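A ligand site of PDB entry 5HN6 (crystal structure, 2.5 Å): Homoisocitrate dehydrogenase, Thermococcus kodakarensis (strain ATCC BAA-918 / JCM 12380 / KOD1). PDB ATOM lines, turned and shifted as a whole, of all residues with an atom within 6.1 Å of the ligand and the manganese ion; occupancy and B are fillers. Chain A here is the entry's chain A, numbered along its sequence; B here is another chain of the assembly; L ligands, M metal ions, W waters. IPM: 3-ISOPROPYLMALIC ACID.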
ATOM      1  N   THR A  71      26.455 -23.782   9.310  1.00  0.00           N
ATOM      2  CA  THR A  71      27.894 -23.593   9.141  1.00  0.00           C
ATOM      3  C   THR A  71      28.564 -24.862   8.631  1.00  0.00           C
ATOM      4  O   THR A  71      28.926 -25.752   9.417  1.00  0.00           O
ATOM      5  CB  THR A  71      28.582 -23.094  10.421  1.00  0.00           C
ATOM      6  OG1 THR A  71      28.012 -21.826  10.790  1.00  0.00           O
ATOM      7  CG2 THR A  71      30.131 -22.961  10.175  1.00  0.00           C
ATOM      8  N   SER A  80      31.810 -18.976  11.489  1.00  0.00           N
ATOM      9  CA  SER A  80      30.408 -19.009  11.982  1.00  0.00           C
ATOM     10  C   SER A  80      29.817 -17.593  12.208  1.00  0.00           C
ATOM     11  O   SER A  80      30.413 -16.770  12.886  1.00  0.00           O
ATOM     12  CB  SER A  80      30.302 -19.786  13.298  1.00  0.00           C
ATOM     13  OG  SER A  80      29.080 -20.504  13.387  1.00  0.00           O
ATOM     14  N   ILE A  82      27.281 -16.643  14.062  1.00  0.00           N
ATOM     15  CA  ILE A  82      27.007 -16.367  15.458  1.00  0.00           C
ATOM     16  C   ILE A  82      28.251 -16.103  16.289  1.00  0.00           C
ATOM     17  O   ILE A  82      28.254 -15.210  17.180  1.00  0.00           O
ATOM     18  CB  ILE A  82      26.081 -17.441  16.085  1.00  0.00           C
ATOM     19  CG1 ILE A  82      25.665 -17.003  17.473  1.00  0.00           C
ATOM     20  CG2 ILE A  82      26.705 -18.825  16.102  1.00  0.00           C
ATOM     21  CD1 ILE A  82      24.882 -15.702  17.480  1.00  0.00           C
ATOM     22  N   LEU A  83      29.333 -16.803  16.007  1.00  0.00           N
ATOM     23  CA  LEU A  83      30.608 -16.488  16.732  1.00  0.00           C
ATOM     24  C   LEU A  83      31.103 -15.095  16.375  1.00  0.00           C
ATOM     25  O   LEU A  83      31.483 -14.308  17.265  1.00  0.00           O
ATOM     26  CB  LEU A  83      31.698 -17.521  16.465  1.00  0.00           C
ATOM     27  CG  LEU A  83      31.281 -18.935  16.910  1.00  0.00           C
ATOM     28  CD1 LEU A  83      32.300 -19.970  16.414  1.00  0.00           C
ATOM     29  CD2 LEU A  83      31.020 -19.070  18.412  1.00  0.00           C
ATOM     30  N   ARG A  86      28.821 -12.608  18.232  1.00  0.00           N
ATOM     31  CA  ARG A  86      29.207 -12.656  19.649  1.00  0.00           C
ATOM     32  C   ARG A  86      30.408 -11.819  19.948  1.00  0.00           C
ATOM     33  O   ARG A  86      30.454 -11.060  20.898  1.00  0.00           O
ATOM     34  CB  ARG A  86      29.476 -14.100  20.094  1.00  0.00           C
ATOM     35  CG  ARG A  86      28.195 -14.897  20.245  1.00  0.00           C
ATOM     36  CD  ARG A  86      28.425 -16.319  20.728  1.00  0.00           C
ATOM     37  NE  ARG A  86      27.193 -17.077  20.607  1.00  0.00           N
ATOM     38  CZ  ARG A  86      27.124 -18.399  20.678  1.00  0.00           C
ATOM     39  NH1 ARG A  86      28.221 -19.123  20.895  1.00  0.00           N
ATOM     40  NH2 ARG A  86      25.932 -19.001  20.557  1.00  0.00           N
ATOM     41  N   ASN A  94      26.095 -15.701  28.080  1.00  0.00           N
ATOM     42  CA  ASN A  94      25.119 -16.503  27.387  1.00  0.00           C
ATOM     43  C   ASN A  94      24.263 -17.168  28.461  1.00  0.00           C
ATOM     44  O   ASN A  94      24.769 -17.929  29.275  1.00  0.00           O
ATOM     45  CB  ASN A  94      25.811 -17.529  26.476  1.00  0.00           C
ATOM     46  CG  ASN A  94      24.837 -18.188  25.515  1.00  0.00           C
ATOM     47  OD1 ASN A  94      23.816 -18.725  25.940  1.00  0.00           O
ATOM     48  ND2 ASN A  94      25.143 -18.156  24.226  1.00  0.00           N
ATOM     49  N   ARG A  96      21.024 -19.442  29.197  1.00  0.00           N
ATOM     50  CA  ARG A  96      20.154 -20.443  28.630  1.00  0.00           C
ATOM     51  C   ARG A  96      19.301 -20.986  29.770  1.00  0.00           C
ATOM     52  O   ARG A  96      19.811 -21.335  30.844  1.00  0.00           O
ATOM     53  CB  ARG A  96      21.013 -21.537  27.990  1.00  0.00           C
ATOM     54  CG  ARG A  96      21.766 -21.010  26.778  1.00  0.00           C
ATOM     55  CD  ARG A  96      22.857 -21.896  26.192  1.00  0.00           C
ATOM     56  NE  ARG A  96      23.262 -21.291  24.931  1.00  0.00           N
ATOM     57  CZ  ARG A  96      23.792 -21.905  23.881  1.00  0.00           C
ATOM     58  NH1 ARG A  96      24.036 -23.229  23.871  1.00  0.00           N
ATOM     59  NH2 ARG A  96      24.108 -21.157  22.810  1.00  0.00           N
ATOM     60  N   ARG A 111      26.551 -19.341  30.691  1.00  0.00           N
ATOM     61  CA  ARG A 111      27.716 -19.768  29.938  1.00  0.00           C
ATOM     62  C   ARG A 111      28.538 -18.554  29.641  1.00  0.00           C
ATOM     63  O   ARG A 111      28.066 -17.664  28.947  1.00  0.00           O
ATOM     64  CB  ARG A 111      27.257 -20.431  28.627  1.00  0.00           C
ATOM     65  CG  ARG A 111      28.325 -20.595  27.571  1.00  0.00           C
ATOM     66  CD  ARG A 111      27.743 -21.210  26.311  1.00  0.00           C
ATOM     67  NE  ARG A 111      28.737 -21.229  25.249  1.00  0.00           N
ATOM     68  CZ  ARG A 111      28.512 -21.655  24.023  1.00  0.00           C
ATOM     69  NH1 ARG A 111      29.503 -21.628  23.127  1.00  0.00           N
ATOM     70  NH2 ARG A 111      27.326 -22.108  23.676  1.00  0.00           N
ATOM     71  N   ASN A 113      30.818 -16.334  27.495  1.00  0.00           N
ATOM     72  CA  ASN A 113      30.567 -16.308  26.051  1.00  0.00           C
ATOM     73  C   ASN A 113      31.606 -15.588  25.214  1.00  0.00           C
ATOM     74  O   ASN A 113      31.415 -15.512  24.021  1.00  0.00           O
ATOM     75  CB  ASN A 113      29.233 -15.616  25.846  1.00  0.00           C
ATOM     76  CG  ASN A 113      28.550 -15.991  24.539  1.00  0.00           C
ATOM     77  OD1 ASN A 113      28.477 -17.157  24.125  1.00  0.00           O
ATOM     78  ND2 ASN A 113      27.951 -14.972  23.927  1.00  0.00           N
ATOM     79  N   TYR A 118      36.970 -20.651  23.311  1.00  0.00           N
ATOM     80  CA  TYR A 118      36.465 -19.840  22.194  1.00  0.00           C
ATOM     81  C   TYR A 118      37.292 -18.558  21.993  1.00  0.00           C
ATOM     82  O   TYR A 118      36.996 -17.752  21.125  1.00  0.00           O
ATOM     83  CB  TYR A 118      34.973 -19.435  22.456  1.00  0.00           C
ATOM     84  CG  TYR A 118      33.992 -20.584  22.287  1.00  0.00           C
ATOM     85  CD1 TYR A 118      33.985 -21.651  23.175  1.00  0.00           C
ATOM     86  CD2 TYR A 118      33.109 -20.620  21.232  1.00  0.00           C
ATOM     87  CE1 TYR A 118      33.118 -22.732  23.010  1.00  0.00           C
ATOM     88  CE2 TYR A 118      32.212 -21.684  21.083  1.00  0.00           C
ATOM     89  CZ  TYR A 118      32.242 -22.739  21.958  1.00  0.00           C
ATOM     90  OH  TYR A 118      31.383 -23.774  21.792  1.00  0.00           O
ATOM     91  N   ASN A 214      33.163 -21.163  28.815  1.00  0.00           N
ATOM     92  CA  ASN A 214      32.478 -21.117  27.536  1.00  0.00           C
ATOM     93  C   ASN A 214      32.112 -22.472  26.942  1.00  0.00           C
ATOM     94  O   ASN A 214      30.937 -22.765  26.749  1.00  0.00           O
ATOM     95  CB  ASN A 214      33.309 -20.304  26.522  1.00  0.00           C
ATOM     96  CG  ASN A 214      32.458 -19.708  25.401  1.00  0.00           C
ATOM     97  OD1 ASN A 214      31.534 -20.334  24.876  1.00  0.00           O
ATOM     98  ND2 ASN A 214      32.783 -18.490  25.041  1.00  0.00           N
ATOM     99  N   LEU A 215      33.100 -23.294  26.661  1.00  0.00           N
ATOM    100  CA  LEU A 215      32.848 -24.613  26.091  1.00  0.00           C
ATOM    101  C   LEU A 215      32.100 -25.555  27.036  1.00  0.00           C
ATOM    102  O   LEU A 215      31.299 -26.334  26.563  1.00  0.00           O
ATOM    103  CB  LEU A 215      34.155 -25.246  25.612  1.00  0.00           C
ATOM    104  CG  LEU A 215      34.031 -26.609  24.976  1.00  0.00           C
ATOM    105  CD1 LEU A 215      33.189 -26.547  23.720  1.00  0.00           C
ATOM    106  CD2 LEU A 215      35.394 -27.173  24.725  1.00  0.00           C
ATOM    107  N   ASP A 218      28.624 -24.565  26.778  1.00  0.00           N
ATOM    108  CA  ASP A 218      28.096 -25.107  25.522  1.00  0.00           C
ATOM    109  C   ASP A 218      27.608 -26.536  25.704  1.00  0.00           C
ATOM    110  O   ASP A 218      26.515 -26.911  25.232  1.00  0.00           O
ATOM    111  CB  ASP A 218      29.169 -25.100  24.403  1.00  0.00           C
ATOM    112  CG  ASP A 218      28.622 -25.629  23.045  1.00  0.00           C
ATOM    113  OD1 ASP A 218      27.614 -25.078  22.498  1.00  0.00           O
ATOM    114  OD2 ASP A 218      29.206 -26.618  22.559  1.00  0.00           O
ATOM    115  N   ILE A 219      28.441 -27.330  26.368  1.00  0.00           N
ATOM    116  CA  ILE A 219      28.165 -28.750  26.523  1.00  0.00           C
ATOM    117  C   ILE A 219      27.022 -28.966  27.518  1.00  0.00           C
ATOM    118  O   ILE A 219      26.095 -29.706  27.227  1.00  0.00           O
ATOM    119  CB  ILE A 219      29.405 -29.493  26.978  1.00  0.00           C
ATOM    120  CG1 ILE A 219      30.469 -29.464  25.878  1.00  0.00           C
ATOM    121  CG2 ILE A 219      29.064 -30.957  27.371  1.00  0.00           C
ATOM    122  CD1 ILE A 219      31.834 -29.888  26.405  1.00  0.00           C
ATOM    123  N   SER A 221      24.580 -27.101  28.317  1.00  0.00           N
ATOM    124  CA  SER A 221      23.308 -26.508  27.968  1.00  0.00           C
ATOM    125  C   SER A 221      22.558 -27.352  26.952  1.00  0.00           C
ATOM    126  O   SER A 221      21.338 -27.407  26.972  1.00  0.00           O
ATOM    127  CB  SER A 221      23.488 -25.050  27.466  1.00  0.00           C
ATOM    128  OG  SER A 221      24.335 -24.939  26.336  1.00  0.00           O
ATOM    129  N   ASP A 222      23.288 -27.991  26.061  1.00  0.00           N
ATOM    130  CA  ASP A 222      22.700 -28.982  25.185  1.00  0.00           C
ATOM    131  C   ASP A 222      22.268 -30.166  26.021  1.00  0.00           C
ATOM    132  O   ASP A 222      21.154 -30.651  25.865  1.00  0.00           O
ATOM    133  CB  ASP A 222      23.696 -29.458  24.165  1.00  0.00           C
ATOM    134  CG  ASP A 222      23.570 -28.759  22.867  1.00  0.00           C
ATOM    135  OD1 ASP A 222      23.326 -27.529  22.842  1.00  0.00           O
ATOM    136  OD2 ASP A 222      23.766 -29.470  21.859  1.00  0.00           O
ATOM    137  N   GLU A 247      18.573 -15.731  20.517  1.00  0.00           N
ATOM    138  CA  GLU A 247      18.445 -16.772  19.521  1.00  0.00           C
ATOM    139  C   GLU A 247      17.999 -18.038  20.176  1.00  0.00           C
ATOM    140  O   GLU A 247      18.359 -18.320  21.330  1.00  0.00           O
ATOM    141  CB  GLU A 247      19.815 -17.028  18.867  1.00  0.00           C
ATOM    142  CG  GLU A 247      20.841 -17.605  19.870  1.00  0.00           C
ATOM    143  CD  GLU A 247      22.164 -17.992  19.251  1.00  0.00           C
ATOM    144  OE1 GLU A 247      23.165 -17.945  20.001  1.00  0.00           O
ATOM    145  OE2 GLU A 247      22.206 -18.308  18.034  1.00  0.00           O
ATOM    146  N   VAL A 249      18.434 -21.801  21.079  1.00  0.00           N
ATOM    147  CA  VAL A 249      19.553 -22.701  21.206  1.00  0.00           C
ATOM    148  C   VAL A 249      19.660 -23.700  20.044  1.00  0.00           C
ATOM    149  O   VAL A 249      20.739 -23.972  19.581  1.00  0.00           O
ATOM    150  CB  VAL A 249      19.543 -23.452  22.550  1.00  0.00           C
ATOM    151  CG1 VAL A 249      20.706 -24.444  22.628  1.00  0.00           C
ATOM    152  CG2 VAL A 249      19.649 -22.444  23.684  1.00  0.00           C
ATOM    153  N   LYS B 163      34.774 -30.875  18.603  1.00  0.00           N
ATOM    154  CA  LYS B 163      34.293 -29.519  18.413  1.00  0.00           C
ATOM    155  C   LYS B 163      35.207 -28.816  17.385  1.00  0.00           C
ATOM    156  O   LYS B 163      35.744 -27.727  17.618  1.00  0.00           O
ATOM    157  CB  LYS B 163      34.289 -28.744  19.727  1.00  0.00           C
ATOM    158  CG  LYS B 163      33.496 -27.409  19.723  1.00  0.00           C
ATOM    159  CD  LYS B 163      31.967 -27.622  19.849  1.00  0.00           C
ATOM    160  CE  LYS B 163      31.144 -26.359  19.507  1.00  0.00           C
ATOM    161  NZ  LYS B 163      29.729 -26.406  20.011  1.00  0.00           N
ATOM    162  N   ASN B 165      34.497 -27.429  14.760  1.00  0.00           N
ATOM    163  CA  ASN B 165      33.940 -26.120  14.357  1.00  0.00           C
ATOM    164  C   ASN B 165      34.522 -24.935  15.124  1.00  0.00           C
ATOM    165  O   ASN B 165      34.402 -23.780  14.706  1.00  0.00           O
ATOM    166  CB  ASN B 165      32.377 -26.120  14.403  1.00  0.00           C
ATOM    167  CG  ASN B 165      31.784 -26.803  15.671  1.00  0.00           C
ATOM    168  OD1 ASN B 165      32.490 -27.545  16.378  1.00  0.00           O
ATOM    169  ND2 ASN B 165      30.494 -26.555  15.962  1.00  0.00           N
ATOM    170  N   VAL B 166      35.116 -25.195  16.275  1.00  0.00           N
ATOM    171  CA  VAL B 166      35.697 -24.144  17.114  1.00  0.00           C
ATOM    172  C   VAL B 166      37.179 -24.396  17.390  1.00  0.00           C
ATOM    173  O   VAL B 166      37.927 -23.436  17.546  1.00  0.00           O
ATOM    174  CB  VAL B 166      34.936 -24.080  18.458  1.00  0.00           C
ATOM    175  CG1 VAL B 166      35.615 -23.124  19.444  1.00  0.00           C
ATOM    176  CG2 VAL B 166      33.494 -23.650  18.249  1.00  0.00           C
ATOM    177  N   ASP B 194      28.705 -31.126  22.006  1.00  0.00           N
ATOM    178  CA  ASP B 194      27.466 -30.668  22.662  1.00  0.00           C
ATOM    179  C   ASP B 194      26.234 -31.482  22.276  1.00  0.00           C
ATOM    180  O   ASP B 194      25.509 -31.978  23.156  1.00  0.00           O
ATOM    181  CB  ASP B 194      27.208 -29.162  22.494  1.00  0.00           C
ATOM    182  CG  ASP B 194      27.170 -28.698  21.027  1.00  0.00           C
ATOM    183  OD1 ASP B 194      27.499 -29.455  20.082  1.00  0.00           O
ATOM    184  OD2 ASP B 194      26.825 -27.501  20.825  1.00  0.00           O
ATOM    185  N   SER B 195      25.982 -31.667  20.973  1.00  0.00           N
ATOM    186  CA  SER B 195      24.782 -32.451  20.600  1.00  0.00           C
ATOM    187  C   SER B 195      24.940 -33.915  20.911  1.00  0.00           C
ATOM    188  O   SER B 195      23.946 -34.593  21.131  1.00  0.00           O
ATOM    189  CB  SER B 195      24.389 -32.262  19.148  1.00  0.00           C
ATOM    190  OG  SER B 195      25.493 -32.070  18.349  1.00  0.00           O
HETATM  191  C1  IPM L   1      25.677 -23.043  20.275  1.00  0.00           C
HETATM  192  C2  IPM L   1      26.357 -23.555  18.989  1.00  0.00           C
HETATM  193  C3  IPM L   1      27.613 -22.711  18.683  1.00  0.00           C
HETATM  194  C4  IPM L   1      28.617 -22.748  19.885  1.00  0.00           C
HETATM  195  C5  IPM L   1      28.361 -23.302  17.451  1.00  0.00           C
HETATM  196  C6  IPM L   1      29.619 -22.447  17.070  1.00  0.00           C
HETATM  197  C7  IPM L   1      27.415 -23.389  16.239  1.00  0.00           C
HETATM  198  O1  IPM L   1      26.810 -24.954  19.153  1.00  0.00           O
HETATM  199  O2  IPM L   1      25.307 -21.870  20.274  1.00  0.00           O
HETATM  200  O3  IPM L   1      25.730 -23.722  21.334  1.00  0.00           O
HETATM  201  O4  IPM L   1      29.447 -23.682  19.880  1.00  0.00           O
HETATM  202  O5  IPM L   1      28.532 -21.897  20.801  1.00  0.00           O
HETATM  203 MN    MN M   1      26.167 -25.717  21.297  1.00  0.00          MN
HETATM  204  O   HOH W   1      24.153 -26.330  20.867  1.00  0.00           O
HETATM  205  O   HOH W   2      25.240 -25.852  23.197  1.00  0.00           O
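An oxygen (O4) of the ligand lies within hydrogen-bond range of the side-chain hydroxyl of Tyr 118 (2.7 Å).
O4 of the ligand lies within salt-bridge range of NZ of Lys 163 of chain B (2.7 Å).
An oxygen (O2) of the ligand lies within salt-bridge range of the guanidinium group of Arg 96 (2.9 Å).
The guanidinium group of Arg 86 lies within salt-bridge range of an oxygen (O5) of the ligand.
The guanidinium group (NH1) of Arg 111 lies within salt-bridge range of an oxygen (O5) of the ligand (2.5 Å).
The backbone carbonyl oxygen of Asp 218 is in hydrogen-bond range of the side-chain hydroxyl of Ser 221 (3.1 Å).
The backbone NH (N) of Ser 195 of chain B sits at hydrogen-bond distance from the side-chain carboxylate (OD2) of Asp 222, at 3.2 Å.
The backbone NH (N) of Arg 111 lies within hydrogen-bond range of the backbone carbonyl oxygen (O) of Asn 94 (2.7 Å).
The guanidinium group (NH2) of Arg 86 lies within salt-bridge range of the side-chain carboxylate (OE1) of Glu 247 (3.0 Å).
The side-chain amide oxygen (OD1) of Asn 165 of chain B sits close to the backbone carbonyl oxygen (O) of Lys 163 of chain B, 3.5 Å away.
The side-chain amide oxygen of Asn 94 sits at hydrogen-bond distance from the guanidinium group of Arg 96.
NH1 of Arg 111 is in hydrogen-bond range of OH of Tyr 118, 3.1 Å away.
OD1 of Asp 218 sits close to NH2 of Arg 111, 3.2 Å away.
Leu 83 touches the ligand.
Of the 23 residues printed, 8 come within 4 Å of the ligand.
Along chain A the residues within 4 Å of the ligand span positions 83 to 218.
The nearest printed residue that does not touch the ligand is Asn 165 of chain B (4.2 Å).
Residues that only touch the manganese ion: Asp 222 and Lys 163 of chain B.
Four residues have an atom within 4 Å of the manganese ion: Asp 218, Asp 222, Lys 163 of chain B and Asp 194 of chain B.
OD2 of Asp 194 of chain B is bound to the manganese ion (2.0 Å).
The side-chain carboxylate (OD1) of Asp 218 is bound to the manganese ion, at 2.0 Å.
The manganese ion is bound by an oxygen (O3) of the ligand.
Water W2 binds the manganese ion, 2.1 Å away.
Water W1 is bound to the manganese ion.
An oxygen (O1) of the ligand binds the manganese ion.
The manganese ion has six donor atoms within binding distance.
Water W2 lies within hydrogen-bond range of the side-chain carboxylate (OD1) of Asp 222 (2.6 Å), the backbone carbonyl oxygen (O) of Asp 218 (2.6 Å), the guanidinium group (NH1) of Arg 96 (3.0 Å) and the side-chain hydroxyl (OG) of Ser 221 (3.4 Å).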
